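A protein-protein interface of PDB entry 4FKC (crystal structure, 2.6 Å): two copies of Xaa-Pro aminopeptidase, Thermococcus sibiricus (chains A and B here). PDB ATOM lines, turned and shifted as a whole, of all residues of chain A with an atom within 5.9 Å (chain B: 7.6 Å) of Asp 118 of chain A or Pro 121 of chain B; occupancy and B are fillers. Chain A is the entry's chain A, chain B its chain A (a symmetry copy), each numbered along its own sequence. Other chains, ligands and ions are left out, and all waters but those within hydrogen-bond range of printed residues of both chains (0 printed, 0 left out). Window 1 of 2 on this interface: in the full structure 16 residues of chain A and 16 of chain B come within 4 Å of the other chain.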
ATOM      1  N   ASN A  41       4.632   9.822 -26.112  1.00  0.00           N
ATOM      2  CA  ASN A  41       3.595   9.666 -27.133  1.00  0.00           C
ATOM      3  C   ASN A  41       4.039   8.774 -28.295  1.00  0.00           C
ATOM      4  O   ASN A  41       3.248   7.968 -28.821  1.00  0.00           O
ATOM      5  CB  ASN A  41       3.142  11.044 -27.596  1.00  0.00           C
ATOM      6  CG  ASN A  41       2.508  11.846 -26.462  1.00  0.00           C
ATOM      7  OD1 ASN A  41       1.770  11.286 -25.657  1.00  0.00           O
ATOM      8  ND2 ASN A  41       2.789  13.145 -26.393  1.00  0.00           N
ATOM      9  N   ILE A 116       1.788  19.439 -32.834  1.00  0.00           N
ATOM     10  CA  ILE A 116       3.218  19.236 -32.689  1.00  0.00           C
ATOM     11  C   ILE A 116       3.532  18.695 -31.288  1.00  0.00           C
ATOM     12  O   ILE A 116       3.075  19.227 -30.276  1.00  0.00           O
ATOM     13  CB  ILE A 116       3.988  20.553 -32.951  1.00  0.00           C
ATOM     14  CG1 ILE A 116       4.487  20.618 -34.383  1.00  0.00           C
ATOM     15  CG2 ILE A 116       5.236  20.623 -32.109  1.00  0.00           C
ATOM     16  CD1 ILE A 116       6.030  20.479 -34.483  1.00  0.00           C
ATOM     17  N   ASP A 117       4.305  17.620 -31.258  1.00  0.00           N
ATOM     18  CA  ASP A 117       4.808  17.044 -30.030  1.00  0.00           C
ATOM     19  C   ASP A 117       5.562  18.073 -29.185  1.00  0.00           C
ATOM     20  O   ASP A 117       6.507  18.700 -29.658  1.00  0.00           O
ATOM     21  CB  ASP A 117       5.743  15.872 -30.347  1.00  0.00           C
ATOM     22  CG  ASP A 117       5.655  14.748 -29.319  1.00  0.00           C
ATOM     23  OD1 ASP A 117       5.149  14.988 -28.199  1.00  0.00           O
ATOM     24  OD2 ASP A 117       6.095  13.617 -29.633  1.00  0.00           O
ATOM     25  N   ASP A 118       5.144  18.201 -27.924  1.00  0.00           N
ATOM     26  CA  ASP A 118       5.726  19.135 -26.968  1.00  0.00           C
ATOM     27  C   ASP A 118       7.201  18.809 -26.751  1.00  0.00           C
ATOM     28  O   ASP A 118       7.972  19.696 -26.423  1.00  0.00           O
ATOM     29  CB  ASP A 118       4.970  19.102 -25.618  1.00  0.00           C
ATOM     30  CG  ASP A 118       3.428  19.257 -25.766  1.00  0.00           C
ATOM     31  OD1 ASP A 118       2.839  18.728 -26.730  1.00  0.00           O
ATOM     32  OD2 ASP A 118       2.782  19.894 -24.895  1.00  0.00           O
ATOM     33  N   THR A 119       7.598  17.547 -26.942  1.00  0.00           N
ATOM     34  CA  THR A 119       8.992  17.164 -26.688  1.00  0.00           C
ATOM     35  C   THR A 119       9.873  17.226 -27.909  1.00  0.00           C
ATOM     36  O   THR A 119      11.036  16.838 -27.840  1.00  0.00           O
ATOM     37  CB  THR A 119       9.153  15.745 -26.071  1.00  0.00           C
ATOM     38  OG1 THR A 119       8.769  14.744 -27.032  1.00  0.00           O
ATOM     39  CG2 THR A 119       8.349  15.601 -24.761  1.00  0.00           C
ATOM     40  N   MET A 120       9.338  17.682 -29.033  1.00  0.00           N
ATOM     41  CA  MET A 120      10.179  17.907 -30.205  1.00  0.00           C
ATOM     42  C   MET A 120      11.251  18.968 -29.913  1.00  0.00           C
ATOM     43  O   MET A 120      10.933  20.051 -29.423  1.00  0.00           O
ATOM     44  CB  MET A 120       9.354  18.330 -31.417  1.00  0.00           C
ATOM     45  CG  MET A 120      10.243  18.572 -32.643  1.00  0.00           C
ATOM     46  SD  MET A 120       9.349  18.772 -34.179  1.00  0.00           S
ATOM     47  CE  MET A 120       8.784  17.105 -34.452  1.00  0.00           C
ATOM     48  N   PRO A 121      12.523  18.663 -30.215  1.00  0.00           N
ATOM     49  CA  PRO A 121      13.553  19.664 -29.926  1.00  0.00           C
ATOM     50  C   PRO A 121      13.411  20.884 -30.828  1.00  0.00           C
ATOM     51  O   PRO A 121      12.988  20.757 -31.986  1.00  0.00           O
ATOM     52  CB  PRO A 121      14.862  18.925 -30.221  1.00  0.00           C
ATOM     53  CG  PRO A 121      14.503  17.468 -30.283  1.00  0.00           C
ATOM     54  CD  PRO A 121      13.096  17.426 -30.778  1.00  0.00           C
ATOM     55  N   VAL A 122      13.759  22.049 -30.292  1.00  0.00           N
ATOM     56  CA  VAL A 122      13.703  23.283 -31.039  1.00  0.00           C
ATOM     57  C   VAL A 122      14.684  23.230 -32.220  1.00  0.00           C
ATOM     58  O   VAL A 122      14.413  23.789 -33.298  1.00  0.00           O
ATOM     59  CB  VAL A 122      13.977  24.504 -30.114  1.00  0.00           C
ATOM     60  CG1 VAL A 122      14.479  25.688 -30.894  1.00  0.00           C
ATOM     61  CG2 VAL A 122      12.715  24.889 -29.365  1.00  0.00           C
ATOM     62  N   PRO A 139       0.317  22.597 -29.600  1.00  0.00           N
ATOM     63  CA  PRO A 139       0.858  21.528 -28.770  1.00  0.00           C
ATOM     64  C   PRO A 139      -0.081  20.336 -28.780  1.00  0.00           C
ATOM     65  O   PRO A 139      -1.304  20.522 -28.775  1.00  0.00           O
ATOM     66  CB  PRO A 139       0.889  22.159 -27.367  1.00  0.00           C
ATOM     67  CG  PRO A 139      -0.116  23.247 -27.403  1.00  0.00           C
ATOM     68  CD  PRO A 139      -0.013  23.794 -28.799  1.00  0.00           C
ATOM     69  N   ILE A 140       0.495  19.138 -28.793  1.00  0.00           N
ATOM     70  CA  ILE A 140      -0.255  17.881 -28.791  1.00  0.00           C
ATOM     71  C   ILE A 140      -0.871  17.526 -27.403  1.00  0.00           C
ATOM     72  O   ILE A 140      -1.913  16.866 -27.322  1.00  0.00           O
ATOM     73  CB  ILE A 140       0.633  16.721 -29.357  1.00  0.00           C
ATOM     74  CG1 ILE A 140      -0.191  15.480 -29.722  1.00  0.00           C
ATOM     75  CG2 ILE A 140       1.781  16.354 -28.410  1.00  0.00           C
ATOM     76  CD1 ILE A 140       0.599  14.457 -30.503  1.00  0.00           C
ATOM     77  N   SER A 141      -0.253  17.994 -26.323  1.00  0.00           N
ATOM     78  CA  SER A 141      -0.581  17.491 -24.998  1.00  0.00           C
ATOM     79  C   SER A 141      -2.063  17.654 -24.603  1.00  0.00           C
ATOM     80  O   SER A 141      -2.654  16.723 -24.084  1.00  0.00           O
ATOM     81  CB  SER A 141       0.380  18.051 -23.934  1.00  0.00           C
ATOM     82  OG  SER A 141       0.133  19.423 -23.655  1.00  0.00           O
ATOM     83  N   PRO A 142      -2.681  18.813 -24.881  1.00  0.00           N
ATOM     84  CA  PRO A 142      -4.109  18.920 -24.512  1.00  0.00           C
ATOM     85  C   PRO A 142      -5.005  17.927 -25.252  1.00  0.00           C
ATOM     86  O   PRO A 142      -6.085  17.594 -24.773  1.00  0.00           O
ATOM     87  CB  PRO A 142      -4.491  20.349 -24.922  1.00  0.00           C
ATOM     88  CG  PRO A 142      -3.184  21.093 -25.015  1.00  0.00           C
ATOM     89  CD  PRO A 142      -2.178  20.058 -25.492  1.00  0.00           C
ATOM     90  N   ALA B  37      18.285  26.290 -22.375  1.00  0.00           N
ATOM     91  CA  ALA B  37      17.263  25.516 -21.686  1.00  0.00           C
ATOM     92  C   ALA B  37      17.977  24.470 -20.823  1.00  0.00           C
ATOM     93  O   ALA B  37      19.178  24.239 -21.013  1.00  0.00           O
ATOM     94  CB  ALA B  37      16.329  24.872 -22.691  1.00  0.00           C
ATOM     95  N   PRO B  38      17.270  23.864 -19.853  1.00  0.00           N
ATOM     96  CA  PRO B  38      17.980  22.884 -19.023  1.00  0.00           C
ATOM     97  C   PRO B  38      18.546  21.781 -19.899  1.00  0.00           C
ATOM     98  O   PRO B  38      17.916  21.413 -20.883  1.00  0.00           O
ATOM     99  CB  PRO B  38      16.887  22.333 -18.111  1.00  0.00           C
ATOM    100  CG  PRO B  38      15.832  23.460 -18.045  1.00  0.00           C
ATOM    101  CD  PRO B  38      15.871  24.071 -19.419  1.00  0.00           C
ATOM    102  N   THR B  53      11.404  19.596 -16.016  1.00  0.00           N
ATOM    103  CA  THR B  53      10.845  20.900 -16.280  1.00  0.00           C
ATOM    104  C   THR B  53      10.056  20.749 -17.588  1.00  0.00           C
ATOM    105  O   THR B  53      10.276  21.473 -18.572  1.00  0.00           O
ATOM    106  CB  THR B  53      11.967  21.987 -16.303  1.00  0.00           C
ATOM    107  OG1 THR B  53      12.853  21.760 -17.404  1.00  0.00           O
ATOM    108  CG2 THR B  53      12.788  21.947 -14.988  1.00  0.00           C
ATOM    109  N   LEU B  54       9.122  19.791 -17.556  1.00  0.00           N
ATOM    110  CA  LEU B  54       8.436  19.268 -18.738  1.00  0.00           C
ATOM    111  C   LEU B  54       8.073  20.358 -19.719  1.00  0.00           C
ATOM    112  O   LEU B  54       8.782  20.602 -20.695  1.00  0.00           O
ATOM    113  N   GLU B  55       6.956  21.011 -19.448  1.00  0.00           N
ATOM    114  CA  GLU B  55       6.531  22.139 -20.236  1.00  0.00           C
ATOM    115  C   GLU B  55       6.613  23.356 -19.298  1.00  0.00           C
ATOM    116  O   GLU B  55       5.975  24.399 -19.557  1.00  0.00           O
ATOM    117  CB  GLU B  55       5.101  21.895 -20.776  1.00  0.00           C
ATOM    118  CG  GLU B  55       4.766  22.420 -22.230  1.00  0.00           C
ATOM    119  CD  GLU B  55       3.389  21.916 -22.738  1.00  0.00           C
ATOM    120  OE1 GLU B  55       2.860  20.958 -22.111  1.00  0.00           O
ATOM    121  OE2 GLU B  55       2.842  22.455 -23.743  1.00  0.00           O
ATOM    122  N   ARG B  56       7.398  23.222 -18.219  1.00  0.00           N
ATOM    123  CA  ARG B  56       7.612  24.312 -17.257  1.00  0.00           C
ATOM    124  C   ARG B  56       8.809  25.195 -17.620  1.00  0.00           C
ATOM    125  O   ARG B  56       9.962  24.745 -17.611  1.00  0.00           O
ATOM    126  CB  ARG B  56       7.776  23.769 -15.840  1.00  0.00           C
ATOM    127  CG  ARG B  56       6.467  23.442 -15.114  1.00  0.00           C
ATOM    128  CD  ARG B  56       6.779  22.879 -13.726  1.00  0.00           C
ATOM    129  NE  ARG B  56       5.613  22.838 -12.837  1.00  0.00           N
ATOM    130  CZ  ARG B  56       5.104  23.875 -12.164  1.00  0.00           C
ATOM    131  NH1 ARG B  56       5.627  25.100 -12.267  1.00  0.00           N
ATOM    132  NH2 ARG B  56       4.043  23.685 -11.387  1.00  0.00           N
ATOM    133  N   PHE B  58      11.847  27.052 -17.764  1.00  0.00           N
ATOM    134  CA  PHE B  58      13.067  27.281 -17.010  1.00  0.00           C
ATOM    135  C   PHE B  58      14.067  27.693 -18.072  1.00  0.00           C
ATOM    136  O   PHE B  58      14.520  26.870 -18.849  1.00  0.00           O
ATOM    137  CB  PHE B  58      13.493  25.998 -16.297  1.00  0.00           C
ATOM    138  CG  PHE B  58      14.432  26.206 -15.125  1.00  0.00           C
ATOM    139  CD1 PHE B  58      15.594  26.970 -15.244  1.00  0.00           C
ATOM    140  CD2 PHE B  58      14.170  25.594 -13.904  1.00  0.00           C
ATOM    141  CE1 PHE B  58      16.460  27.129 -14.157  1.00  0.00           C
ATOM    142  CE2 PHE B  58      15.028  25.743 -12.814  1.00  0.00           C
ATOM    143  CZ  PHE B  58      16.177  26.509 -12.945  1.00  0.00           C
ATOM    144  N   TYR B  97       5.373  33.517 -19.509  1.00  0.00           N
ATOM    145  CA  TYR B  97       5.725  34.019 -20.828  1.00  0.00           C
ATOM    146  C   TYR B  97       5.573  35.537 -20.942  1.00  0.00           C
ATOM    147  O   TYR B  97       6.298  36.178 -21.710  1.00  0.00           O
ATOM    148  CB  TYR B  97       5.008  33.225 -21.920  1.00  0.00           C
ATOM    149  CG  TYR B  97       5.449  31.758 -21.946  1.00  0.00           C
ATOM    150  CD1 TYR B  97       6.480  31.328 -22.788  1.00  0.00           C
ATOM    151  CD2 TYR B  97       4.844  30.802 -21.116  1.00  0.00           C
ATOM    152  CE1 TYR B  97       6.887  29.996 -22.809  1.00  0.00           C
ATOM    153  CE2 TYR B  97       5.256  29.468 -21.126  1.00  0.00           C
ATOM    154  CZ  TYR B  97       6.273  29.077 -21.978  1.00  0.00           C
ATOM    155  OH  TYR B  97       6.680  27.767 -21.995  1.00  0.00           O
ATOM    156  N   ILE B 116      19.572  29.976 -29.792  1.00  0.00           N
ATOM    157  CA  ILE B 116      18.596  29.167 -29.084  1.00  0.00           C
ATOM    158  C   ILE B 116      19.156  27.759 -28.845  1.00  0.00           C
ATOM    159  O   ILE B 116      19.668  27.106 -29.756  1.00  0.00           O
ATOM    160  CB  ILE B 116      17.266  29.098 -29.874  1.00  0.00           C
ATOM    161  CG1 ILE B 116      16.275  30.129 -29.364  1.00  0.00           C
ATOM    162  CG2 ILE B 116      16.581  27.773 -29.659  1.00  0.00           C
ATOM    163  CD1 ILE B 116      15.083  29.486 -28.606  1.00  0.00           C
ATOM    164  N   ASP B 117      19.063  27.318 -27.600  1.00  0.00           N
ATOM    165  CA  ASP B 117      19.422  25.972 -27.210  1.00  0.00           C
ATOM    166  C   ASP B 117      18.678  24.922 -28.037  1.00  0.00           C
ATOM    167  O   ASP B 117      17.450  24.924 -28.094  1.00  0.00           O
ATOM    168  CB  ASP B 117      19.110  25.756 -25.726  1.00  0.00           C
ATOM    169  CG  ASP B 117      20.113  24.838 -25.035  1.00  0.00           C
ATOM    170  OD1 ASP B 117      20.843  24.101 -25.735  1.00  0.00           O
ATOM    171  OD2 ASP B 117      20.173  24.855 -23.783  1.00  0.00           O
ATOM    172  N   ASP B 118      19.446  24.012 -28.641  1.00  0.00           N
ATOM    173  CA  ASP B 118      18.926  22.940 -29.480  1.00  0.00           C
ATOM    174  C   ASP B 118      18.000  22.040 -28.666  1.00  0.00           C
ATOM    175  O   ASP B 118      17.105  21.432 -29.228  1.00  0.00           O
ATOM    176  CB  ASP B 118      20.072  22.104 -30.099  1.00  0.00           C
ATOM    177  CG  ASP B 118      21.157  22.966 -30.807  1.00  0.00           C
ATOM    178  OD1 ASP B 118      21.490  24.067 -30.325  1.00  0.00           O
ATOM    179  OD2 ASP B 118      21.713  22.532 -31.848  1.00  0.00           O
ATOM    180  N   THR B 119      18.205  21.963 -27.348  1.00  0.00           N
ATOM    181  CA  THR B 119      17.384  21.066 -26.524  1.00  0.00           C
ATOM    182  C   THR B 119      16.177  21.731 -25.915  1.00  0.00           C
ATOM    183  O   THR B 119      15.469  21.106 -25.131  1.00  0.00           O
ATOM    184  CB  THR B 119      18.168  20.379 -25.369  1.00  0.00           C
ATOM    185  OG1 THR B 119      18.561  21.360 -24.391  1.00  0.00           O
ATOM    186  CG2 THR B 119      19.388  19.595 -25.898  1.00  0.00           C
ATOM    187  N   MET B 120      15.941  22.995 -26.239  1.00  0.00           N
ATOM    188  CA  MET B 120      14.708  23.643 -25.802  1.00  0.00           C
ATOM    189  C   MET B 120      13.478  22.933 -26.389  1.00  0.00           C
ATOM    190  O   MET B 120      13.415  22.702 -27.596  1.00  0.00           O
ATOM    191  CB  MET B 120      14.682  25.119 -26.188  1.00  0.00           C
ATOM    192  CG  MET B 120      13.382  25.795 -25.734  1.00  0.00           C
ATOM    193  SD  MET B 120      13.386  27.578 -25.867  1.00  0.00           S
ATOM    194  CE  MET B 120      14.507  28.005 -24.551  1.00  0.00           C
ATOM    195  N   PRO B 121      12.499  22.587 -25.539  1.00  0.00           N
ATOM    196  CA  PRO B 121      11.330  21.896 -26.089  1.00  0.00           C
ATOM    197  C   PRO B 121      10.513  22.816 -26.988  1.00  0.00           C
ATOM    198  O   PRO B 121      10.448  24.030 -26.744  1.00  0.00           O
ATOM    199  CB  PRO B 121      10.528  21.506 -24.844  1.00  0.00           C
ATOM    200  CG  PRO B 121      11.470  21.661 -23.686  1.00  0.00           C
ATOM    201  CD  PRO B 121      12.405  22.756 -24.077  1.00  0.00           C
ATOM    202  N   VAL B 122       9.903  22.235 -28.016  1.00  0.00           N
ATOM    203  CA  VAL B 122       9.071  22.978 -28.933  1.00  0.00           C
ATOM    204  C   VAL B 122       7.855  23.556 -28.193  1.00  0.00           C
ATOM    205  O   VAL B 122       7.380  24.660 -28.515  1.00  0.00           O
ATOM    206  CB  VAL B 122       8.647  22.092 -30.140  1.00  0.00           C
ATOM    207  CG1 VAL B 122       7.386  22.600 -30.784  1.00  0.00           C
ATOM    208  CG2 VAL B 122       9.758  22.043 -31.171  1.00  0.00           C
ATOM    209  N   GLY B 123       7.377  22.809 -27.195  1.00  0.00           N
ATOM    210  CA  GLY B 123       6.221  23.196 -26.395  1.00  0.00           C
ATOM    211  C   GLY B 123       6.419  24.558 -25.760  1.00  0.00           C
ATOM    212  O   GLY B 123       5.511  25.398 -25.758  1.00  0.00           O
ATOM    213  N   VAL B 124       7.618  24.779 -25.229  1.00  0.00           N
ATOM    214  CA  VAL B 124       8.004  26.086 -24.701  1.00  0.00           C
ATOM    215  C   VAL B 124       8.194  27.079 -25.852  1.00  0.00           C
ATOM    216  O   VAL B 124       7.790  28.232 -25.757  1.00  0.00           O
ATOM    217  CB  VAL B 124       9.263  25.982 -23.804  1.00  0.00           C
ATOM    218  CG1 VAL B 124       9.839  27.351 -23.494  1.00  0.00           C
ATOM    219  CG2 VAL B 124       8.939  25.226 -22.535  1.00  0.00           C
ATOM    220  N   PHE B 125       8.781  26.628 -26.953  1.00  0.00           N
ATOM    221  CA  PHE B 125       8.955  27.517 -28.097  1.00  0.00           C
ATOM    222  C   PHE B 125       7.634  28.166 -28.503  1.00  0.00           C
ATOM    223  O   PHE B 125       7.590  29.368 -28.765  1.00  0.00           O
ATOM    224  CB  PHE B 125       9.542  26.751 -29.277  1.00  0.00           C
ATOM    225  CG  PHE B 125       9.969  27.623 -30.425  1.00  0.00           C
ATOM    226  CD1 PHE B 125       9.050  28.045 -31.382  1.00  0.00           C
ATOM    227  CD2 PHE B 125      11.296  27.999 -30.567  1.00  0.00           C
ATOM    228  CE1 PHE B 125       9.449  28.837 -32.441  1.00  0.00           C
ATOM    229  CE2 PHE B 125      11.699  28.789 -31.623  1.00  0.00           C
ATOM    230  CZ  PHE B 125      10.781  29.204 -32.561  1.00  0.00           C
ATOM    231  N   LEU B 126       6.562  27.366 -28.532  1.00  0.00           N
ATOM    232  CA  LEU B 126       5.280  27.800 -29.087  1.00  0.00           C
ATOM    233  C   LEU B 126       4.602  28.893 -28.267  1.00  0.00           C
ATOM    234  O   LEU B 126       4.154  29.912 -28.810  1.00  0.00           O
ATOM    235  CB  LEU B 126       4.342  26.607 -29.287  1.00  0.00           C
ATOM    236  CG  LEU B 126       4.712  25.594 -30.386  1.00  0.00           C
ATOM    237  CD1 LEU B 126       3.997  24.299 -30.151  1.00  0.00           C
ATOM    238  CD2 LEU B 126       4.378  26.129 -31.748  1.00  0.00           C
ATOM    239  N   LYS B 127       4.546  28.693 -26.953  1.00  0.00           N
ATOM    240  CA  LYS B 127       3.961  29.686 -26.059  1.00  0.00           C
ATOM    241  C   LYS B 127       4.656  31.040 -26.183  1.00  0.00           C
ATOM    242  O   LYS B 127       4.015  32.103 -26.097  1.00  0.00           O
ATOM    243  CB  LYS B 127       3.980  29.175 -24.627  1.00  0.00           C
ATOM    244  CG  LYS B 127       2.813  28.258 -24.332  1.00  0.00           C
ATOM    245  CD  LYS B 127       3.056  27.366 -23.144  1.00  0.00           C
ATOM    246  CE  LYS B 127       1.884  26.408 -22.969  1.00  0.00           C
ATOM    247  NZ  LYS B 127       2.403  25.084 -22.529  1.00  0.00           N
ATOM    248  N   PHE B 132       9.586  35.245 -29.927  1.00  0.00           N
ATOM    249  CA  PHE B 132      10.586  34.719 -30.890  1.00  0.00           C
ATOM    250  C   PHE B 132      10.388  35.169 -32.346  1.00  0.00           C
ATOM    251  O   PHE B 132      11.365  35.344 -33.096  1.00  0.00           O
ATOM    252  CB  PHE B 132      10.684  33.189 -30.808  1.00  0.00           C
ATOM    253  CG  PHE B 132      11.205  32.669 -29.488  1.00  0.00           C
ATOM    254  CD1 PHE B 132      11.081  31.320 -29.174  1.00  0.00           C
ATOM    255  CD2 PHE B 132      11.814  33.517 -28.565  1.00  0.00           C
ATOM    256  CE1 PHE B 132      11.559  30.811 -27.970  1.00  0.00           C
ATOM    257  CE2 PHE B 132      12.288  33.031 -27.358  1.00  0.00           C
ATOM    258  CZ  PHE B 132      12.163  31.666 -27.058  1.00  0.00           C
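Of the 21 printed residues of chain B, 8 touch a printed residue of chain A. Printed residues of chain A that touch a printed residue of chain B: Ile 116, Asp 118, Met 120, Pro 121, Val 122 and Ser 141. Along chain A the printed residues that touch a printed residue of chain B span positions 116 to 141. Among the printed residues, no Asp or Glu carboxylate lies within 4 Å of a Lys or Arg side-chain nitrogen of the other chain.
Asp 118 of chain A touches four residues of chain B. Printed residues of chain B within 4 Å of Met 120 of chain A: Pro 121 (3.7 Å) and Val 122 (2.8 Å). Printed residues of chain B within 4 Å of Ser 141 of chain A: Glu 55 (3.5 Å). Of the printed residues of chain A, Glu 55 of chain B touches Asp 118 and Ser 141. Arg 56 of chain B touches none of the printed residues of chain A. Printed residues of chain A within 4 Å of Met 120 of chain B: Pro 121 and Val 122. Of chain A, only Asp 118 (3.5 Å), Met 120 (3.7 Å) and Val 122 (3.6 Å) come within 4 Å of Pro 121 of chain B. Of the printed residues of chain A, Val 122 of chain B touches Ile 116, Asp 118, Met 120 and Pro 121. The nearest residue of chain B that does not touch Asp 118 of chain A is Val 124 of chain B (5.2 Å). The nearest printed residue of chain A that does not touch Pro 121 of chain B is Thr 119 of chain A (5.0 Å). The nearest printed residue of chain A that does not touch Glu 55 of chain B is Pro 139 of chain A (4.1 Å).
N of Val 122 of chain A sits at hydrogen-bond distance from O of Met 120 of chain B (2.8 Å). OG of Ser 141 of chain A sits at hydrogen-bond distance from OE1 of Glu 55 of chain B, at 3.5 Å. The backbone carbonyl oxygen (O) of Asp 118 of chain A sits at hydrogen-bond distance from the backbone NH (N) of Gly 123 of chain B, at 3.3 Å. OE2 of Glu 55 of chain B sits close to OD2 of Asp 118 of chain A, at 2.8 Å. The backbone carbonyl oxygen of Met 120 of chain A sits at hydrogen-bond distance from the backbone NH of Val 122 of chain B (2.8 Å).
Ile 116 of chain A touches Val 122 of chain B, and with the chains exchanged Val 122 of chain A touches Ile 116 of chain B. Asp 118 of chain A touches Pro 121 of chain B, and with the chains exchanged Pro 121 of chain A touches Asp 118 of chain B. Met 120 of chain A touches Pro 121 of chain B, and with the chains exchanged Pro 121 of chain A touches Met 120 of chain B. Pro 121 of chain A touches Val 122 of chain B, and with the chains exchanged Val 122 of chain A touches Pro 121 of chain B. 7 positions are printed for both chains.
Among the printed residues, merely in contact across the chains: Ile 116 of chain A with Val 122 of chain B (3.2 Å), Asp 118 of chain A with Pro 121 of chain B (3.5 Å), Asp 118 of chain A with Val 122 of chain B (3.6 Å), Met 120 of chain A with Pro 121 of chain B (3.7 Å), Pro 121 of chain A with Asp 118 of chain B (3.5 Å), Pro 121 of chain A with Met 120 of chain B (3.7 Å), Pro 121 of chain A with Val 122 of chain B (3.6 Å), Val 122 of chain A with Ile 116 of chain B (3.2 Å), Val 122 of chain A with Asp 118 of chain B (3.6 Å), Val 122 of chain A with Pro 121 of chain B (3.6 Å) and Val 122 of chain A with Phe 125 of chain B (3.6 Å).
The backbone carbonyl oxygen (O) of Ile 116 of chain A is in hydrogen-bond range of the backbone NH (N) of Ile 140 of chain A (3.0 Å). OD1 of Asp 118 of chain A sits close to N of Ile 140 of chain A (3.1 Å). NZ of Lys 127 of chain B lies within salt-bridge range of OE2 of Glu 55 of chain B (2.9 Å). OD2 of Asp 118 of chain A sits at hydrogen-bond distance from OG of Ser 141 of chain A, at 3.0 Å.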
